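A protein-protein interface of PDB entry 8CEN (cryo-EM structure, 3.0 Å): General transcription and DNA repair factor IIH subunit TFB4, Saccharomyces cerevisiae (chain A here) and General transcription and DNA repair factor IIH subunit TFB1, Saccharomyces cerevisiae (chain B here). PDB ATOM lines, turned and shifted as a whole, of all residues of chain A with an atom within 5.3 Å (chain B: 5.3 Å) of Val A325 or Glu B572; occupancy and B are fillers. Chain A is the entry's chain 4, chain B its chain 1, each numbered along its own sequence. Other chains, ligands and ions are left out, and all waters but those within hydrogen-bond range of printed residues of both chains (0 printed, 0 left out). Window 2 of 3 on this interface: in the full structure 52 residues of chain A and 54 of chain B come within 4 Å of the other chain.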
ATOM      1  N   ARG A 322       3.352 -14.926 -22.991  1.00  0.00           N
ATOM      2  CA  ARG A 322       2.800 -16.125 -23.612  1.00  0.00           C
ATOM      3  C   ARG A 322       1.301 -16.240 -23.350  1.00  0.00           C
ATOM      4  O   ARG A 322       0.797 -15.827 -22.301  1.00  0.00           O
ATOM      5  CB  ARG A 322       3.506 -17.395 -23.126  1.00  0.00           C
ATOM      6  CG  ARG A 322       3.282 -17.748 -21.665  1.00  0.00           C
ATOM      7  CD  ARG A 322       4.016 -19.024 -21.288  1.00  0.00           C
ATOM      8  NE  ARG A 322       5.465 -18.908 -21.379  1.00  0.00           N
ATOM      9  CZ  ARG A 322       6.189 -19.496 -22.322  1.00  0.00           C
ATOM     10  NH1 ARG A 322       5.628 -20.234 -23.264  1.00  0.00           N
ATOM     11  NH2 ARG A 322       7.508 -19.338 -22.321  1.00  0.00           N
ATOM     12  N   LYS A 323       0.596 -16.770 -24.326  1.00  0.00           N
ATOM     13  CA  LYS A 323      -0.826 -17.061 -24.363  1.00  0.00           C
ATOM     14  C   LYS A 323      -1.069 -18.489 -23.877  1.00  0.00           C
ATOM     15  O   LYS A 323      -0.201 -19.355 -24.025  1.00  0.00           O
ATOM     16  CB  LYS A 323      -1.358 -16.896 -25.786  1.00  0.00           C
ATOM     17  CG  LYS A 323      -2.685 -16.156 -25.897  1.00  0.00           C
ATOM     18  CD  LYS A 323      -2.496 -14.654 -25.757  1.00  0.00           C
ATOM     19  CE  LYS A 323      -3.745 -13.897 -26.180  1.00  0.00           C
ATOM     20  NZ  LYS A 323      -3.570 -12.423 -26.059  1.00  0.00           N
ATOM     21  N   PRO A 324      -2.223 -18.770 -23.273  1.00  0.00           N
ATOM     22  CA  PRO A 324      -2.508 -20.139 -22.829  1.00  0.00           C
ATOM     23  C   PRO A 324      -2.718 -21.085 -24.003  1.00  0.00           C
ATOM     24  O   PRO A 324      -2.941 -20.679 -25.146  1.00  0.00           O
ATOM     25  CB  PRO A 324      -3.784 -19.991 -21.996  1.00  0.00           C
ATOM     26  CG  PRO A 324      -4.367 -18.690 -22.406  1.00  0.00           C
ATOM     27  CD  PRO A 324      -3.206 -17.814 -22.741  1.00  0.00           C
ATOM     28  N   VAL A 325      -2.645 -22.376 -23.696  1.00  0.00           N
ATOM     29  CA  VAL A 325      -2.615 -23.425 -24.706  1.00  0.00           C
ATOM     30  C   VAL A 325      -3.923 -24.202 -24.692  1.00  0.00           C
ATOM     31  O   VAL A 325      -4.532 -24.431 -23.638  1.00  0.00           O
ATOM     32  CB  VAL A 325      -1.415 -24.369 -24.494  1.00  0.00           C
ATOM     33  CG1 VAL A 325      -0.134 -23.672 -24.889  1.00  0.00           C
ATOM     34  CG2 VAL A 325      -1.342 -24.824 -23.046  1.00  0.00           C
ATOM     35  N   VAL A 326      -4.351 -24.607 -25.884  1.00  0.00           N
ATOM     36  CA  VAL A 326      -5.538 -25.434 -26.095  1.00  0.00           C
ATOM     37  C   VAL A 326      -5.406 -26.079 -27.474  1.00  0.00           C
ATOM     38  O   VAL A 326      -4.890 -25.442 -28.405  1.00  0.00           O
ATOM     39  CB  VAL A 326      -6.830 -24.606 -25.927  1.00  0.00           C
ATOM     40  CG1 VAL A 326      -6.908 -23.477 -26.930  1.00  0.00           C
ATOM     41  CG2 VAL A 326      -8.067 -25.478 -26.041  1.00  0.00           C
ATOM     42  N   PRO A 327      -5.776 -27.348 -27.636  1.00  0.00           N
ATOM     43  CA  PRO A 327      -5.724 -27.967 -28.965  1.00  0.00           C
ATOM     44  C   PRO A 327      -6.727 -27.344 -29.924  1.00  0.00           C
ATOM     45  O   PRO A 327      -7.739 -26.765 -29.526  1.00  0.00           O
ATOM     46  CB  PRO A 327      -6.067 -29.435 -28.693  1.00  0.00           C
ATOM     47  CG  PRO A 327      -5.704 -29.651 -27.278  1.00  0.00           C
ATOM     48  CD  PRO A 327      -5.942 -28.351 -26.570  1.00  0.00           C
ATOM     49  N   HIS B 567      -0.766 -26.561 -16.305  1.00  0.00           N
ATOM     50  CA  HIS B 567      -0.620 -26.936 -17.710  1.00  0.00           C
ATOM     51  C   HIS B 567      -1.223 -25.897 -18.652  1.00  0.00           C
ATOM     52  O   HIS B 567      -0.791 -25.783 -19.804  1.00  0.00           O
ATOM     53  CB  HIS B 567      -1.240 -28.310 -17.947  1.00  0.00           C
ATOM     54  CG  HIS B 567      -0.335 -29.444 -17.578  1.00  0.00           C
ATOM     55  ND1 HIS B 567       0.738 -29.819 -18.357  1.00  0.00           N
ATOM     56  CD2 HIS B 567      -0.332 -30.274 -16.508  1.00  0.00           C
ATOM     57  CE1 HIS B 567       1.359 -30.837 -17.788  1.00  0.00           C
ATOM     58  NE2 HIS B 567       0.729 -31.132 -16.666  1.00  0.00           N
ATOM     59  N   PHE B 568      -2.204 -25.128 -18.181  1.00  0.00           N
ATOM     60  CA  PHE B 568      -2.844 -24.100 -18.993  1.00  0.00           C
ATOM     61  C   PHE B 568      -1.968 -22.859 -19.119  1.00  0.00           C
ATOM     62  O   PHE B 568      -1.925 -22.234 -20.184  1.00  0.00           O
ATOM     63  CB  PHE B 568      -4.202 -23.758 -18.374  1.00  0.00           C
ATOM     64  CG  PHE B 568      -5.143 -23.043 -19.297  1.00  0.00           C
ATOM     65  CD1 PHE B 568      -5.737 -23.710 -20.356  1.00  0.00           C
ATOM     66  CD2 PHE B 568      -5.487 -21.721 -19.066  1.00  0.00           C
ATOM     67  CE1 PHE B 568      -6.621 -23.058 -21.196  1.00  0.00           C
ATOM     68  CE2 PHE B 568      -6.376 -21.066 -19.896  1.00  0.00           C
ATOM     69  CZ  PHE B 568      -6.941 -21.734 -20.964  1.00  0.00           C
ATOM     70  N   SER B 570       1.394 -22.897 -18.571  1.00  0.00           N
ATOM     71  CA  SER B 570       2.749 -23.215 -19.013  1.00  0.00           C
ATOM     72  C   SER B 570       3.044 -22.650 -20.397  1.00  0.00           C
ATOM     73  O   SER B 570       4.190 -22.281 -20.681  1.00  0.00           O
ATOM     74  CB  SER B 570       2.962 -24.728 -19.006  1.00  0.00           C
ATOM     75  OG  SER B 570       1.992 -25.381 -19.806  1.00  0.00           O
ATOM     76  N   GLY B 571       2.036 -22.568 -21.259  1.00  0.00           N
ATOM     77  CA  GLY B 571       2.203 -21.989 -22.581  1.00  0.00           C
ATOM     78  C   GLY B 571       3.074 -22.780 -23.535  1.00  0.00           C
ATOM     79  O   GLY B 571       3.862 -22.186 -24.283  1.00  0.00           O
ATOM     80  N   GLU B 572       2.953 -24.106 -23.529  1.00  0.00           N
ATOM     81  CA  GLU B 572       3.686 -24.971 -24.446  1.00  0.00           C
ATOM     82  C   GLU B 572       2.699 -25.789 -25.267  1.00  0.00           C
ATOM     83  O   GLU B 572       1.797 -26.422 -24.710  1.00  0.00           O
ATOM     84  CB  GLU B 572       4.646 -25.892 -23.686  1.00  0.00           C
ATOM     85  CG  GLU B 572       5.524 -25.174 -22.670  1.00  0.00           C
ATOM     86  CD  GLU B 572       6.460 -24.162 -23.307  1.00  0.00           C
ATOM     87  OE1 GLU B 572       6.933 -24.408 -24.438  1.00  0.00           O
ATOM     88  OE2 GLU B 572       6.720 -23.115 -22.678  1.00  0.00           O
ATOM     89  N   GLN B 573       2.876 -25.775 -26.591  1.00  0.00           N
ATOM     90  CA  GLN B 573       1.976 -26.499 -27.483  1.00  0.00           C
ATOM     91  C   GLN B 573       2.169 -28.009 -27.424  1.00  0.00           C
ATOM     92  O   GLN B 573       1.278 -28.749 -27.850  1.00  0.00           O
ATOM     93  CB  GLN B 573       2.166 -26.020 -28.924  1.00  0.00           C
ATOM     94  CG  GLN B 573       1.680 -24.605 -29.195  1.00  0.00           C
ATOM     95  CD  GLN B 573       0.174 -24.473 -29.074  1.00  0.00           C
ATOM     96  OE1 GLN B 573      -0.333 -23.843 -28.149  1.00  0.00           O
ATOM     97  NE2 GLN B 573      -0.549 -25.070 -30.014  1.00  0.00           N
ATOM     98  N   LYS B 574       3.309 -28.483 -26.912  1.00  0.00           N
ATOM     99  CA  LYS B 574       3.588 -29.915 -26.897  1.00  0.00           C
ATOM    100  C   LYS B 574       2.744 -30.668 -25.877  1.00  0.00           C
ATOM    101  O   LYS B 574       2.593 -31.889 -25.997  1.00  0.00           O
ATOM    102  CB  LYS B 574       5.072 -30.156 -26.616  1.00  0.00           C
ATOM    103  CG  LYS B 574       5.565 -29.526 -25.324  1.00  0.00           C
ATOM    104  CD  LYS B 574       7.052 -29.763 -25.125  1.00  0.00           C
ATOM    105  CE  LYS B 574       7.522 -29.211 -23.789  1.00  0.00           C
ATOM    106  NZ  LYS B 574       6.843 -29.877 -22.644  1.00  0.00           N
ATOM    107  N   GLN B 575       2.194 -29.973 -24.882  1.00  0.00           N
ATOM    108  CA  GLN B 575       1.434 -30.588 -23.802  1.00  0.00           C
ATOM    109  C   GLN B 575      -0.036 -30.165 -23.815  1.00  0.00           C
ATOM    110  O   GLN B 575      -0.749 -30.335 -22.818  1.00  0.00           O
ATOM    111  CB  GLN B 575       2.145 -30.294 -22.474  1.00  0.00           C
ATOM    112  CG  GLN B 575       2.266 -28.823 -22.062  1.00  0.00           C
ATOM    113  CD  GLN B 575       1.060 -28.278 -21.342  1.00  0.00           C
ATOM    114  OE1 GLN B 575       0.360 -29.013 -20.651  1.00  0.00           O
ATOM    115  NE2 GLN B 575       0.809 -26.984 -21.496  1.00  0.00           N
ATOM    116  N   ALA B 576      -0.517 -29.672 -24.961  1.00  0.00           N
ATOM    117  CA  ALA B 576      -1.932 -29.343 -25.103  1.00  0.00           C
ATOM    118  C   ALA B 576      -2.817 -30.583 -25.020  1.00  0.00           C
ATOM    119  O   ALA B 576      -3.985 -30.477 -24.637  1.00  0.00           O
ATOM    120  CB  ALA B 576      -2.170 -28.610 -26.422  1.00  0.00           C
ATOM    121  N   VAL B 579      -3.345 -30.868 -21.479  1.00  0.00           N
ATOM    122  CA  VAL B 579      -4.315 -29.825 -21.132  1.00  0.00           C
ATOM    123  C   VAL B 579      -5.739 -30.284 -21.436  1.00  0.00           C
ATOM    124  O   VAL B 579      -6.658 -30.081 -20.632  1.00  0.00           O
ATOM    125  CB  VAL B 579      -3.979 -28.511 -21.866  1.00  0.00           C
ATOM    126  CG1 VAL B 579      -5.033 -27.453 -21.588  1.00  0.00           C
ATOM    127  CG2 VAL B 579      -2.625 -28.004 -21.441  1.00  0.00           C
ATOM    128  N   TYR B 630     -11.076 -22.190 -20.865  1.00  0.00           N
ATOM    129  CA  TYR B 630     -10.656 -23.183 -21.850  1.00  0.00           C
ATOM    130  C   TYR B 630     -11.512 -23.099 -23.106  1.00  0.00           C
ATOM    131  O   TYR B 630     -10.990 -23.102 -24.226  1.00  0.00           O
ATOM    132  CB  TYR B 630     -10.729 -24.585 -21.238  1.00  0.00           C
ATOM    133  CG  TYR B 630     -10.219 -25.708 -22.125  1.00  0.00           C
ATOM    134  CD1 TYR B 630     -11.066 -26.372 -23.008  1.00  0.00           C
ATOM    135  CD2 TYR B 630      -8.893 -26.121 -22.059  1.00  0.00           C
ATOM    136  CE1 TYR B 630     -10.605 -27.396 -23.812  1.00  0.00           C
ATOM    137  CE2 TYR B 630      -8.425 -27.151 -22.857  1.00  0.00           C
ATOM    138  CZ  TYR B 630      -9.286 -27.786 -23.728  1.00  0.00           C
ATOM    139  OH  TYR B 630      -8.827 -28.807 -24.527  1.00  0.00           O
ATOM    140  N   TYR B 637      -9.072 -19.807 -30.892  1.00  0.00           N
ATOM    141  CA  TYR B 637      -8.127 -20.412 -31.829  1.00  0.00           C
ATOM    142  C   TYR B 637      -8.786 -21.145 -32.996  1.00  0.00           C
ATOM    143  O   TYR B 637      -8.155 -21.265 -34.051  1.00  0.00           O
ATOM    144  CB  TYR B 637      -7.154 -21.358 -31.117  1.00  0.00           C
ATOM    145  CG  TYR B 637      -6.161 -20.672 -30.203  1.00  0.00           C
ATOM    146  CD1 TYR B 637      -5.955 -19.299 -30.267  1.00  0.00           C
ATOM    147  CD2 TYR B 637      -5.388 -21.404 -29.314  1.00  0.00           C
ATOM    148  CE1 TYR B 637      -5.037 -18.675 -29.444  1.00  0.00           C
ATOM    149  CE2 TYR B 637      -4.469 -20.790 -28.485  1.00  0.00           C
ATOM    150  CZ  TYR B 637      -4.297 -19.426 -28.557  1.00  0.00           C
ATOM    151  OH  TYR B 637      -3.381 -18.810 -27.738  1.00  0.00           O
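The backbone carbonyl oxygen of Gly B571 is in hydrogen-bond range of the guanidinium group of Arg A322.
The side-chain carboxylate (OE2) of Glu B572 lies within salt-bridge range of the guanidinium group (NH1) of Arg A322 (3.1 Å).
The side-chain hydroxyl (OH) of Tyr B637 sits at hydrogen-bond distance from the backbone carbonyl oxygen (O) of Pro A324 (3.2 Å).
The side-chain hydroxyl (OG) of Ser B570 is in hydrogen-bond range of the backbone carbonyl oxygen (O) of His B567, at 2.8 Å.
A ring nitrogen (ND1) of His B567 lies within hydrogen-bond range of the side-chain amide oxygen (OE1) of Gln B575 (2.5 Å).
NE2 of Gln B575 is in hydrogen-bond range of OG of Ser B570 (2.6 Å).
NE2 of Gln B575 sits at hydrogen-bond distance from O of Glu B572 (3.4 Å).
Among the printed residues, merely in contact across the chains: Arg A322 with Ser B570, Lys A323 with Gly B571, Lys A323 with Tyr B637, Pro A324 with Phe B568, Val A325 with His B567, Val A325 with Phe B568, Val A325 with Gly B571, Val A325 with Glu B572, Val A325 with Gln B573, Val A325 with Gln B575, Val A325 with Val B579, Val A326 with Tyr B630, Val A326 with Tyr B637, Pro A327 with Ala B576 and Pro A327 with Tyr B630.
Val A325 touches just these residues of chain B: His B567, Phe B568, Gly B571, Glu B572, Gln B573, Gln B575 and Val B579.
Printed residues of chain B within 4 Å of Val A326: Tyr B630 and Tyr B637.
Of the printed residues of chain A, Gly B571 touches Arg A322, Lys A323 and Val A325.
Printed residues of chain A within 4 Å of Glu B572: Arg A322 and Val A325.
Printed residues of chain A within 4 Å of Ala B576: Pro A327 (3.3 Å).
The nearest residue of chain B that does not touch Val A325 is Ser B570 (4.7 Å).
The nearest printed residue of chain A that does not touch Glu B572 is Lys A323 (5.7 Å).
The nearest printed residue of chain B that does not touch Pro A324 is Gly B571 (5.1 Å).
Of the 6 printed residues of chain A, 6 touch a printed residue of chain B.
Hydrophobic or aromatic side chains of chain A within 4 Å of the printed part of chain B: Pro A324, Val A325, Val A326 and Pro A327.
Printed residues of chain B that touch a printed residue of chain A: His B567, Phe B568, Ser B570, Gly B571, Glu B572, Gln B573, Gln B575, Ala B576, Val B579, Tyr B630 and Tyr B637.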
